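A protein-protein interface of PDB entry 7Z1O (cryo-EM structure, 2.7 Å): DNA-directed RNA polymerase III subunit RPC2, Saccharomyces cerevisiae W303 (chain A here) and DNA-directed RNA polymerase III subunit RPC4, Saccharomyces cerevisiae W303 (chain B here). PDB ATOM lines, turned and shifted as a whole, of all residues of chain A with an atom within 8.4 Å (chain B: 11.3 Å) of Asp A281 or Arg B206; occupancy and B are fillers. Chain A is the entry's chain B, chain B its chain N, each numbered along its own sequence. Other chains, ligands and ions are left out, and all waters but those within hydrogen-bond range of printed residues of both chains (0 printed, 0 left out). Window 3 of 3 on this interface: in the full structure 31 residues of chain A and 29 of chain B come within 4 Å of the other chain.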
ATOM      1  N   GLY A 238       9.937  -1.168   1.309  1.00  0.00           N
ATOM      2  CA  GLY A 238       9.584  -1.459  -0.064  1.00  0.00           C
ATOM      3  C   GLY A 238       9.072  -0.275  -0.853  1.00  0.00           C
ATOM      4  O   GLY A 238       8.664  -0.448  -2.007  1.00  0.00           O
ATOM      5  N   MET A 269       5.412   5.734 -14.554  1.00  0.00           N
ATOM      6  CA  MET A 269       5.856   4.346 -14.624  1.00  0.00           C
ATOM      7  C   MET A 269       6.723   4.103 -15.854  1.00  0.00           C
ATOM      8  O   MET A 269       7.720   3.375 -15.782  1.00  0.00           O
ATOM      9  CB  MET A 269       4.644   3.414 -14.621  1.00  0.00           C
ATOM     10  CG  MET A 269       4.950   1.992 -15.033  1.00  0.00           C
ATOM     11  SD  MET A 269       3.581   1.242 -15.920  1.00  0.00           S
ATOM     12  CE  MET A 269       3.986   1.768 -17.582  1.00  0.00           C
ATOM     13  N   CYS A 273      10.273   2.810 -15.002  1.00  0.00           N
ATOM     14  CA  CYS A 273      10.437   1.403 -15.342  1.00  0.00           C
ATOM     15  C   CYS A 273      10.648   1.166 -16.827  1.00  0.00           C
ATOM     16  O   CYS A 273      11.635   0.538 -17.219  1.00  0.00           O
ATOM     17  CB  CYS A 273       9.217   0.605 -14.867  1.00  0.00           C
ATOM     18  SG  CYS A 273       8.639   1.061 -13.229  1.00  0.00           S
ATOM     19  N   GLY A 274       9.745   1.647 -17.666  1.00  0.00           N
ATOM     20  CA  GLY A 274       9.841   1.408 -19.095  1.00  0.00           C
ATOM     21  C   GLY A 274       9.041   0.186 -19.497  1.00  0.00           C
ATOM     22  O   GLY A 274       7.865   0.070 -19.156  1.00  0.00           O
ATOM     23  N   ASN A 275       9.683  -0.724 -20.222  1.00  0.00           N
ATOM     24  CA  ASN A 275       9.027  -1.921 -20.720  1.00  0.00           C
ATOM     25  C   ASN A 275       9.360  -3.169 -19.913  1.00  0.00           C
ATOM     26  O   ASN A 275       8.985  -4.271 -20.324  1.00  0.00           O
ATOM     27  CB  ASN A 275       9.397  -2.143 -22.188  1.00  0.00           C
ATOM     28  CG  ASN A 275       8.494  -1.384 -23.131  1.00  0.00           C
ATOM     29  OD1 ASN A 275       8.047  -0.279 -22.823  1.00  0.00           O
ATOM     30  ND2 ASN A 275       8.217  -1.970 -24.285  1.00  0.00           N
ATOM     31  N   ASP A 276      10.049  -3.028 -18.784  1.00  0.00           N
ATOM     32  CA  ASP A 276      10.453  -4.171 -17.977  1.00  0.00           C
ATOM     33  C   ASP A 276       9.366  -4.502 -16.962  1.00  0.00           C
ATOM     34  O   ASP A 276       8.901  -3.624 -16.230  1.00  0.00           O
ATOM     35  CB  ASP A 276      11.775  -3.884 -17.267  1.00  0.00           C
ATOM     36  CG  ASP A 276      12.434  -5.138 -16.732  1.00  0.00           C
ATOM     37  OD1 ASP A 276      11.895  -6.241 -16.961  1.00  0.00           O
ATOM     38  OD2 ASP A 276      13.495  -5.022 -16.083  1.00  0.00           O
ATOM     39  N   SER A 277       8.967  -5.776 -16.922  1.00  0.00           N
ATOM     40  CA  SER A 277       7.896  -6.190 -16.024  1.00  0.00           C
ATOM     41  C   SER A 277       8.360  -6.225 -14.573  1.00  0.00           C
ATOM     42  O   SER A 277       7.583  -5.916 -13.662  1.00  0.00           O
ATOM     43  CB  SER A 277       7.358  -7.556 -16.445  1.00  0.00           C
ATOM     44  OG  SER A 277       8.279  -8.583 -16.126  1.00  0.00           O
ATOM     45  N   SER A 278       9.617  -6.612 -14.337  1.00  0.00           N
ATOM     46  CA  SER A 278      10.129  -6.687 -12.972  1.00  0.00           C
ATOM     47  C   SER A 278      10.201  -5.307 -12.328  1.00  0.00           C
ATOM     48  O   SER A 278       9.837  -5.139 -11.156  1.00  0.00           O
ATOM     49  CB  SER A 278      11.503  -7.354 -12.967  1.00  0.00           C
ATOM     50  OG  SER A 278      11.507  -8.511 -13.784  1.00  0.00           O
ATOM     51  N   TYR A 279      10.662  -4.306 -13.083  1.00  0.00           N
ATOM     52  CA  TYR A 279      10.728  -2.948 -12.554  1.00  0.00           C
ATOM     53  C   TYR A 279       9.336  -2.406 -12.263  1.00  0.00           C
ATOM     54  O   TYR A 279       9.129  -1.717 -11.259  1.00  0.00           O
ATOM     55  CB  TYR A 279      11.466  -2.032 -13.531  1.00  0.00           C
ATOM     56  CG  TYR A 279      12.913  -2.397 -13.780  1.00  0.00           C
ATOM     57  CD1 TYR A 279      13.617  -3.196 -12.889  1.00  0.00           C
ATOM     58  CD2 TYR A 279      13.576  -1.937 -14.906  1.00  0.00           C
ATOM     59  CE1 TYR A 279      14.936  -3.529 -13.119  1.00  0.00           C
ATOM     60  CE2 TYR A 279      14.894  -2.264 -15.144  1.00  0.00           C
ATOM     61  CZ  TYR A 279      15.568  -3.058 -14.248  1.00  0.00           C
ATOM     62  OH  TYR A 279      16.883  -3.384 -14.482  1.00  0.00           O
ATOM     63  N   GLN A 280       8.367  -2.710 -13.132  1.00  0.00           N
ATOM     64  CA  GLN A 280       6.989  -2.294 -12.883  1.00  0.00           C
ATOM     65  C   GLN A 280       6.426  -2.966 -11.639  1.00  0.00           C
ATOM     66  O   GLN A 280       5.721  -2.329 -10.850  1.00  0.00           O
ATOM     67  CB  GLN A 280       6.116  -2.601 -14.098  1.00  0.00           C
ATOM     68  CG  GLN A 280       6.398  -1.724 -15.299  1.00  0.00           C
ATOM     69  CD  GLN A 280       5.482  -2.022 -16.464  1.00  0.00           C
ATOM     70  OE1 GLN A 280       4.600  -2.874 -16.370  1.00  0.00           O
ATOM     71  NE2 GLN A 280       5.684  -1.319 -17.571  1.00  0.00           N
ATOM     72  N   ASP A 281       6.727  -4.253 -11.446  1.00  0.00           N
ATOM     73  CA  ASP A 281       6.255  -4.955 -10.257  1.00  0.00           C
ATOM     74  C   ASP A 281       6.867  -4.372  -8.990  1.00  0.00           C
ATOM     75  O   ASP A 281       6.204  -4.296  -7.949  1.00  0.00           O
ATOM     76  CB  ASP A 281       6.572  -6.446 -10.367  1.00  0.00           C
ATOM     77  CG  ASP A 281       5.747  -7.141 -11.431  1.00  0.00           C
ATOM     78  OD1 ASP A 281       4.613  -6.690 -11.693  1.00  0.00           O
ATOM     79  OD2 ASP A 281       6.234  -8.136 -12.007  1.00  0.00           O
ATOM     80  N   ILE A 282       8.135  -3.961  -9.057  1.00  0.00           N
ATOM     81  CA  ILE A 282       8.773  -3.351  -7.893  1.00  0.00           C
ATOM     82  C   ILE A 282       8.191  -1.966  -7.618  1.00  0.00           C
ATOM     83  O   ILE A 282       7.928  -1.606  -6.464  1.00  0.00           O
ATOM     84  CB  ILE A 282      10.299  -3.303  -8.090  1.00  0.00           C
ATOM     85  CG1 ILE A 282      10.880  -4.716  -8.088  1.00  0.00           C
ATOM     86  CG2 ILE A 282      10.962  -2.475  -7.007  1.00  0.00           C
ATOM     87  CD1 ILE A 282      12.317  -4.783  -8.548  1.00  0.00           C
ATOM     88  N   PHE A 283       7.959  -1.175  -8.667  1.00  0.00           N
ATOM     89  CA  PHE A 283       7.596   0.229  -8.523  1.00  0.00           C
ATOM     90  C   PHE A 283       6.092   0.472  -8.410  1.00  0.00           C
ATOM     91  O   PHE A 283       5.688   1.593  -8.081  1.00  0.00           O
ATOM     92  CB  PHE A 283       8.166   1.016  -9.712  1.00  0.00           C
ATOM     93  CG  PHE A 283       8.015   2.505  -9.595  1.00  0.00           C
ATOM     94  CD1 PHE A 283       8.692   3.208  -8.615  1.00  0.00           C
ATOM     95  CD2 PHE A 283       7.194   3.199 -10.464  1.00  0.00           C
ATOM     96  CE1 PHE A 283       8.551   4.576  -8.505  1.00  0.00           C
ATOM     97  CE2 PHE A 283       7.052   4.565 -10.358  1.00  0.00           C
ATOM     98  CZ  PHE A 283       7.731   5.254  -9.379  1.00  0.00           C
ATOM     99  N   ALA A 284       5.254  -0.545  -8.636  1.00  0.00           N
ATOM    100  CA  ALA A 284       3.808  -0.333  -8.635  1.00  0.00           C
ATOM    101  C   ALA A 284       3.255   0.034  -7.264  1.00  0.00           C
ATOM    102  O   ALA A 284       2.110   0.491  -7.176  1.00  0.00           O
ATOM    103  CB  ALA A 284       3.100  -1.581  -9.160  1.00  0.00           C
ATOM    104  N   VAL A 285       4.028  -0.166  -6.195  1.00  0.00           N
ATOM    105  CA  VAL A 285       3.567   0.207  -4.861  1.00  0.00           C
ATOM    106  C   VAL A 285       3.443   1.721  -4.738  1.00  0.00           C
ATOM    107  O   VAL A 285       2.486   2.236  -4.149  1.00  0.00           O
ATOM    108  CB  VAL A 285       4.513  -0.370  -3.792  1.00  0.00           C
ATOM    109  CG1 VAL A 285       4.005  -0.051  -2.396  1.00  0.00           C
ATOM    110  CG2 VAL A 285       4.672  -1.867  -3.980  1.00  0.00           C
ATOM    111  N   ASN A 286       4.404   2.457  -5.302  1.00  0.00           N
ATOM    112  CA  ASN A 286       4.455   3.902  -5.093  1.00  0.00           C
ATOM    113  C   ASN A 286       3.372   4.638  -5.873  1.00  0.00           C
ATOM    114  O   ASN A 286       3.063   5.791  -5.552  1.00  0.00           O
ATOM    115  CB  ASN A 286       5.834   4.435  -5.474  1.00  0.00           C
ATOM    116  CG  ASN A 286       6.956   3.675  -4.803  1.00  0.00           C
ATOM    117  OD1 ASN A 286       7.363   4.003  -3.691  1.00  0.00           O
ATOM    118  ND2 ASN A 286       7.462   2.650  -5.478  1.00  0.00           N
ATOM    119  N   VAL A 357      15.362   1.611  -8.447  1.00  0.00           N
ATOM    120  CA  VAL A 357      14.612   0.402  -8.788  1.00  0.00           C
ATOM    121  C   VAL A 357      15.545  -0.680  -9.325  1.00  0.00           C
ATOM    122  O   VAL A 357      15.422  -1.862  -8.974  1.00  0.00           O
ATOM    123  CB  VAL A 357      13.489   0.742  -9.787  1.00  0.00           C
ATOM    124  CG1 VAL A 357      12.961  -0.507 -10.465  1.00  0.00           C
ATOM    125  CG2 VAL A 357      12.362   1.468  -9.083  1.00  0.00           C
ATOM    126  N   TYR A 361      16.214  -4.411  -7.753  1.00  0.00           N
ATOM    127  CA  TYR A 361      16.034  -5.667  -8.477  1.00  0.00           C
ATOM    128  C   TYR A 361      17.227  -6.594  -8.277  1.00  0.00           C
ATOM    129  O   TYR A 361      17.062  -7.774  -7.947  1.00  0.00           O
ATOM    130  CB  TYR A 361      15.802  -5.407  -9.964  1.00  0.00           C
ATOM    131  CG  TYR A 361      15.645  -6.684 -10.760  1.00  0.00           C
ATOM    132  CD1 TYR A 361      14.568  -7.532 -10.540  1.00  0.00           C
ATOM    133  CD2 TYR A 361      16.579  -7.049 -11.719  1.00  0.00           C
ATOM    134  CE1 TYR A 361      14.422  -8.704 -11.257  1.00  0.00           C
ATOM    135  CE2 TYR A 361      16.441  -8.219 -12.441  1.00  0.00           C
ATOM    136  CZ  TYR A 361      15.361  -9.041 -12.206  1.00  0.00           C
ATOM    137  OH  TYR A 361      15.214 -10.208 -12.921  1.00  0.00           O
ATOM    138  N   VAL B 202      -6.259   1.062 -20.273  1.00  0.00           N
ATOM    139  CA  VAL B 202      -4.969   0.946 -20.938  1.00  0.00           C
ATOM    140  C   VAL B 202      -4.080  -0.013 -20.162  1.00  0.00           C
ATOM    141  O   VAL B 202      -3.792   0.199 -18.977  1.00  0.00           O
ATOM    142  CB  VAL B 202      -4.308   2.324 -21.080  1.00  0.00           C
ATOM    143  CG1 VAL B 202      -3.001   2.204 -21.838  1.00  0.00           C
ATOM    144  CG2 VAL B 202      -5.242   3.282 -21.790  1.00  0.00           C
ATOM    145  N   ARG B 203      -3.637  -1.074 -20.830  1.00  0.00           N
ATOM    146  CA  ARG B 203      -2.679  -1.996 -20.252  1.00  0.00           C
ATOM    147  C   ARG B 203      -1.287  -1.683 -20.777  1.00  0.00           C
ATOM    148  O   ARG B 203      -1.074  -1.686 -21.998  1.00  0.00           O
ATOM    149  CB  ARG B 203      -3.054  -3.454 -20.565  1.00  0.00           C
ATOM    150  CG  ARG B 203      -3.467  -3.727 -22.005  1.00  0.00           C
ATOM    151  CD  ARG B 203      -4.402  -4.921 -22.097  1.00  0.00           C
ATOM    152  NE  ARG B 203      -5.758  -4.590 -21.678  1.00  0.00           N
ATOM    153  CZ  ARG B 203      -6.836  -5.288 -22.009  1.00  0.00           C
ATOM    154  NH1 ARG B 203      -6.752  -6.371 -22.766  1.00  0.00           N
ATOM    155  NH2 ARG B 203      -8.027  -4.892 -21.570  1.00  0.00           N
ATOM    156  N   PRO B 204      -0.337  -1.367 -19.903  1.00  0.00           N
ATOM    157  CA  PRO B 204       1.017  -1.059 -20.370  1.00  0.00           C
ATOM    158  C   PRO B 204       1.705  -2.278 -20.959  1.00  0.00           C
ATOM    159  O   PRO B 204       1.438  -3.419 -20.579  1.00  0.00           O
ATOM    160  CB  PRO B 204       1.725  -0.585 -19.097  1.00  0.00           C
ATOM    161  CG  PRO B 204       0.973  -1.237 -17.990  1.00  0.00           C
ATOM    162  CD  PRO B 204      -0.456  -1.252 -18.442  1.00  0.00           C
ATOM    163  N   VAL B 205       2.603  -2.017 -21.910  1.00  0.00           N
ATOM    164  CA  VAL B 205       3.379  -3.094 -22.511  1.00  0.00           C
ATOM    165  C   VAL B 205       4.393  -3.611 -21.499  1.00  0.00           C
ATOM    166  O   VAL B 205       5.058  -2.836 -20.799  1.00  0.00           O
ATOM    167  CB  VAL B 205       4.025  -2.616 -23.823  1.00  0.00           C
ATOM    168  CG1 VAL B 205       4.967  -1.442 -23.593  1.00  0.00           C
ATOM    169  CG2 VAL B 205       4.755  -3.763 -24.507  1.00  0.00           C
ATOM    170  N   ARG B 206       4.476  -4.933 -21.378  1.00  0.00           N
ATOM    171  CA  ARG B 206       5.323  -5.578 -20.385  1.00  0.00           C
ATOM    172  C   ARG B 206       6.200  -6.614 -21.068  1.00  0.00           C
ATOM    173  O   ARG B 206       5.696  -7.484 -21.785  1.00  0.00           O
ATOM    174  CB  ARG B 206       4.482  -6.241 -19.289  1.00  0.00           C
ATOM    175  CG  ARG B 206       3.669  -5.269 -18.457  1.00  0.00           C
ATOM    176  CD  ARG B 206       2.605  -5.992 -17.650  1.00  0.00           C
ATOM    177  NE  ARG B 206       3.184  -6.847 -16.621  1.00  0.00           N
ATOM    178  CZ  ARG B 206       3.424  -6.461 -15.376  1.00  0.00           C
ATOM    179  NH1 ARG B 206       3.146  -5.234 -14.967  1.00  0.00           N
ATOM    180  NH2 ARG B 206       3.956  -7.328 -14.519  1.00  0.00           N
ATOM    181  N   VAL B 207       7.508  -6.517 -20.844  1.00  0.00           N
ATOM    182  CA  VAL B 207       8.477  -7.477 -21.355  1.00  0.00           C
ATOM    183  C   VAL B 207       9.280  -8.005 -20.177  1.00  0.00           C
ATOM    184  O   VAL B 207       9.595  -7.256 -19.245  1.00  0.00           O
ATOM    185  CB  VAL B 207       9.413  -6.853 -22.413  1.00  0.00           C
ATOM    186  CG1 VAL B 207      10.238  -7.934 -23.094  1.00  0.00           C
ATOM    187  CG2 VAL B 207       8.625  -6.061 -23.441  1.00  0.00           C
ATOM    188  N   ARG B 208       9.596  -9.298 -20.209  1.00  0.00           N
ATOM    189  CA  ARG B 208      10.428  -9.892 -19.172  1.00  0.00           C
ATOM    190  C   ARG B 208      11.831  -9.298 -19.210  1.00  0.00           C
ATOM    191  O   ARG B 208      12.291  -8.795 -20.238  1.00  0.00           O
ATOM    192  CB  ARG B 208      10.492 -11.409 -19.345  1.00  0.00           C
ATOM    193  CG  ARG B 208       9.198 -12.128 -19.006  1.00  0.00           C
ATOM    194  CD  ARG B 208       9.362 -13.634 -19.122  1.00  0.00           C
ATOM    195  NE  ARG B 208       9.510 -14.061 -20.507  1.00  0.00           N
ATOM    196  CZ  ARG B 208      10.638 -14.514 -21.036  1.00  0.00           C
ATOM    197  NH1 ARG B 208      11.748 -14.607 -20.321  1.00  0.00           N
ATOM    198  NH2 ARG B 208      10.655 -14.881 -22.314  1.00  0.00           N
ATOM    199  N   HIS B 209      12.508  -9.354 -18.060  1.00  0.00           N
ATOM    200  CA  HIS B 209      13.813  -8.712 -17.930  1.00  0.00           C
ATOM    201  C   HIS B 209      14.869  -9.404 -18.782  1.00  0.00           C
ATOM    202  O   HIS B 209      15.822  -8.764 -19.244  1.00  0.00           O
ATOM    203  CB  HIS B 209      14.237  -8.689 -16.462  1.00  0.00           C
ATOM    204  CG  HIS B 209      15.500  -7.929 -16.210  1.00  0.00           C
ATOM    205  ND1 HIS B 209      15.570  -6.556 -16.293  1.00  0.00           N
ATOM    206  CD2 HIS B 209      16.742  -8.350 -15.881  1.00  0.00           C
ATOM    207  CE1 HIS B 209      16.802  -6.163 -16.023  1.00  0.00           C
ATOM    208  NE2 HIS B 209      17.533  -7.233 -15.770  1.00  0.00           N
ATOM    209  N   GLU B 210      14.722 -10.713 -18.999  1.00  0.00           N
ATOM    210  CA  GLU B 210      15.716 -11.445 -19.779  1.00  0.00           C
ATOM    211  C   GLU B 210      15.652 -11.088 -21.258  1.00  0.00           C
ATOM    212  O   GLU B 210      16.665 -11.181 -21.961  1.00  0.00           O
ATOM    213  CB  GLU B 210      15.526 -12.950 -19.589  1.00  0.00           C
ATOM    214  CG  GLU B 210      15.923 -13.466 -18.214  1.00  0.00           C
ATOM    215  CD  GLU B 210      14.808 -13.336 -17.194  1.00  0.00           C
ATOM    216  OE1 GLU B 210      13.699 -12.904 -17.573  1.00  0.00           O
ATOM    217  OE2 GLU B 210      15.040 -13.669 -16.013  1.00  0.00           O
ATOM    218  N   ASP B 211      14.481 -10.681 -21.750  1.00  0.00           N
ATOM    219  CA  ASP B 211      14.283 -10.396 -23.166  1.00  0.00           C
ATOM    220  C   ASP B 211      14.014  -8.920 -23.437  1.00  0.00           C
ATOM    221  O   ASP B 211      13.445  -8.582 -24.478  1.00  0.00           O
ATOM    222  CB  ASP B 211      13.140 -11.248 -23.720  1.00  0.00           C
ATOM    223  CG  ASP B 211      13.365 -12.733 -23.514  1.00  0.00           C
ATOM    224  OD1 ASP B 211      14.535 -13.144 -23.361  1.00  0.00           O
ATOM    225  OD2 ASP B 211      12.372 -13.490 -23.506  1.00  0.00           O
ATOM    226  N   VAL B 212      14.410  -8.033 -22.522  1.00  0.00           N
ATOM    227  CA  VAL B 212      14.134  -6.610 -22.704  1.00  0.00           C
ATOM    228  C   VAL B 212      15.043  -6.019 -23.779  1.00  0.00           C
ATOM    229  O   VAL B 212      14.687  -5.036 -24.439  1.00  0.00           O
ATOM    230  CB  VAL B 212      14.258  -5.866 -21.358  1.00  0.00           C
ATOM    231  CG1 VAL B 212      15.702  -5.840 -20.868  1.00  0.00           C
ATOM    232  CG2 VAL B 212      13.683  -4.458 -21.454  1.00  0.00           C
ATOM    233  N   GLU B 213      16.217  -6.617 -23.990  1.00  0.00           N
ATOM    234  CA  GLU B 213      17.146  -6.096 -24.985  1.00  0.00           C
ATOM    235  C   GLU B 213      16.898  -6.675 -26.372  1.00  0.00           C
ATOM    236  O   GLU B 213      17.222  -6.030 -27.374  1.00  0.00           O
ATOM    237  CB  GLU B 213      18.588  -6.365 -24.545  1.00  0.00           C
ATOM    238  CG  GLU B 213      18.899  -7.825 -24.247  1.00  0.00           C
ATOM    239  CD  GLU B 213      19.447  -8.568 -25.449  1.00  0.00           C
ATOM    240  OE1 GLU B 213      19.929  -7.904 -26.390  1.00  0.00           O
ATOM    241  OE2 GLU B 213      19.398  -9.816 -25.452  1.00  0.00           O
ATOM    242  N   THR B 214      16.329  -7.878 -26.453  1.00  0.00           N
ATOM    243  CA  THR B 214      16.066  -8.515 -27.736  1.00  0.00           C
ATOM    244  C   THR B 214      14.792  -7.998 -28.395  1.00  0.00           C
ATOM    245  O   THR B 214      14.740  -7.884 -29.626  1.00  0.00           O
ATOM    246  CB  THR B 214      15.974 -10.035 -27.553  1.00  0.00           C
ATOM    247  OG1 THR B 214      17.115 -10.495 -26.816  1.00  0.00           O
ATOM    248  CG2 THR B 214      15.945 -10.747 -28.899  1.00  0.00           C
ATOM    249  N   VAL B 215      13.775  -7.654 -27.600  1.00  0.00           N
ATOM    250  CA  VAL B 215      12.482  -7.240 -28.142  1.00  0.00           C
ATOM    251  C   VAL B 215      12.524  -5.845 -28.747  1.00  0.00           C
ATOM    252  O   VAL B 215      11.625  -5.489 -29.521  1.00  0.00           O
ATOM    253  CB  VAL B 215      11.423  -7.318 -27.022  1.00  0.00           C
ATOM    254  CG1 VAL B 215      11.692  -6.258 -25.958  1.00  0.00           C
ATOM    255  CG2 VAL B 215       9.991  -7.262 -27.562  1.00  0.00           C
ATOM    256  N   LYS B 216      13.565  -5.060 -28.446  1.00  0.00           N
ATOM    257  CA  LYS B 216      13.603  -3.655 -28.851  1.00  0.00           C
ATOM    258  C   LYS B 216      13.591  -3.506 -30.367  1.00  0.00           C
ATOM    259  O   LYS B 216      13.004  -2.554 -30.899  1.00  0.00           O
ATOM    260  CB  LYS B 216      14.838  -2.978 -28.258  1.00  0.00           C
ATOM    261  CG  LYS B 216      14.711  -2.649 -26.782  1.00  0.00           C
ATOM    262  CD  LYS B 216      16.002  -2.071 -26.228  1.00  0.00           C
ATOM    263  CE  LYS B 216      15.797  -1.506 -24.833  1.00  0.00           C
ATOM    264  NZ  LYS B 216      16.872  -1.937 -23.900  1.00  0.00           N
ATOM    265  N   GLU B 218      12.007  -5.482 -32.439  1.00  0.00           N
ATOM    266  CA  GLU B 218      10.616  -5.663 -32.839  1.00  0.00           C
ATOM    267  C   GLU B 218       9.767  -4.458 -32.449  1.00  0.00           C
ATOM    268  O   GLU B 218       8.885  -4.039 -33.207  1.00  0.00           O
ATOM    269  CB  GLU B 218      10.056  -6.942 -32.217  1.00  0.00           C
ATOM    270  CG  GLU B 218       8.611  -7.239 -32.585  1.00  0.00           C
ATOM    271  CD  GLU B 218       8.177  -8.630 -32.169  1.00  0.00           C
ATOM    272  OE1 GLU B 218       8.967  -9.323 -31.494  1.00  0.00           O
ATOM    273  OE2 GLU B 218       7.045  -9.030 -32.515  1.00  0.00           O
ATOM    274  N   ILE B 219      10.026  -3.884 -31.270  1.00  0.00           N
ATOM    275  CA  ILE B 219       9.194  -2.796 -30.759  1.00  0.00           C
ATOM    276  C   ILE B 219       9.386  -1.531 -31.587  1.00  0.00           C
ATOM    277  O   ILE B 219       8.424  -0.801 -31.866  1.00  0.00           O
ATOM    278  CB  ILE B 219       9.502  -2.560 -29.267  1.00  0.00           C
ATOM    279  CG1 ILE B 219       9.079  -3.780 -28.449  1.00  0.00           C
ATOM    280  CG2 ILE B 219       8.796  -1.315 -28.751  1.00  0.00           C
ATOM    281  CD1 ILE B 219       9.239  -3.606 -26.966  1.00  0.00           C
ATOM    282  N   LEU B 223       6.193   0.251 -33.443  1.00  0.00           N
ATOM    283  CA  LEU B 223       5.718   1.589 -33.114  1.00  0.00           C
ATOM    284  C   LEU B 223       5.520   2.466 -34.345  1.00  0.00           C
ATOM    285  O   LEU B 223       5.220   3.655 -34.205  1.00  0.00           O
ATOM    286  CB  LEU B 223       6.677   2.274 -32.139  1.00  0.00           C
ATOM    287  CG  LEU B 223       6.753   1.691 -30.727  1.00  0.00           C
ATOM    288  CD1 LEU B 223       7.721   2.491 -29.876  1.00  0.00           C
ATOM    289  CD2 LEU B 223       5.373   1.644 -30.087  1.00  0.00           C
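The backbone carbonyl oxygen (O) of Met A269 sits close to the side-chain sulfur (SG) of Cys A273, 3.6 Å away.
O of Met A269 lies within hydrogen-bond range of N of Gly A274, 3.3 Å away.
The side-chain amide nitrogen (NE2) of Gln A280 lies close to the side-chain sulfur (SD) of Met A269 (3.7 Å).
The side-chain sulfur (SG) of Cys A273 lies within hydrogen-bond range of the backbone carbonyl oxygen (O) of Tyr A279, at 3.4 Å.
O of Gly A274 lies within hydrogen-bond range of NE2 of Gln A280 (3.0 Å).
N of Ser A278 lies close to OD1 of Asp A276.
NH1 of Arg B206 is in hydrogen-bond range of OE1 of Gln A280.
The guanidinium group (NH2) of Arg B206 is in salt-bridge range of the side-chain carboxylate (OD1) of Asp A281.
The backbone NH (N) of Val B207 sits at hydrogen-bond distance from the backbone carbonyl oxygen (O) of Asn A275 (2.7 Å).
The backbone NH of Ser A277 is in hydrogen-bond range of the backbone carbonyl oxygen of Val B207 (2.8 Å).
ND1 of His B209 lies within hydrogen-bond range of OD2 of Asp A276 (2.6 Å).
The side-chain carboxylate (OD1) of Asp A276 sits close to the backbone carbonyl oxygen (O) of Val B207 (3.4 Å).
Of chain B, only Val B205 (3.4 Å), Arg B206 (3.7 Å), Val B207 (2.7 Å) and Ile B219 (3.3 Å) come within 4 Å of Asn A275.
Ser A277 touches just these residues of chain B: Arg B206 (3.9 Å), Val B207 (2.8 Å) and Arg B208 (3.95 Å).
Of chain B, only His B209 (3.8 Å) comes within 4 Å of Ser A278.
No residue of chain B comes within 4 Å of Ile A282.
No residue of chain B comes within 4 Å of Ala A284.
Of the printed residues of chain B, Tyr A361 touches His B209.
Of the printed residues of chain A, Arg B206 touches Asn A275 (3.7 Å), Ser A277 (3.9 Å), Gln A280 (3.1 Å) and Asp A281 (3.0 Å).
Of the printed residues of chain A, Val B207 touches Asn A275 (2.7 Å), Asp A276 (3.4 Å) and Ser A277 (2.8 Å).
Glu B210 touches none of the printed residues of chain A.
Val B215 touches none of the printed residues of chain A.
Met A269 touches Pro B204.
Val B205 touches Asn A275 (CG1 to ND2, 3.4 Å).
Arg B206 touches Asn A275 (C to O, 3.7 Å).
CD1 of Ile B219 touches ND2 of Asn A275, at 3.3 Å.
Ser A277 touches Arg B206 (CB to NH2, 3.9 Å).
Arg B208 touches Ser A277 (CA to OG, 3.95 Å).
CB of His B209 touches OG of Ser A278 (3.8 Å).
Tyr A279 touches His B209 (OH to CE1, 3.2 Å).
Val B205 touches Gln A280 (O to NE2, 3.6 Å).
Tyr A361 touches His B209.
Of the 18 printed residues of chain A, 9 touch a printed residue of chain B.
Of the 18 printed residues of chain B, 7 touch a printed residue of chain A.
Printed residues of chain B that touch a printed residue of chain A: Pro B204, Val B205, Arg B206, Val B207, Arg B208, His B209 and Ile B219.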
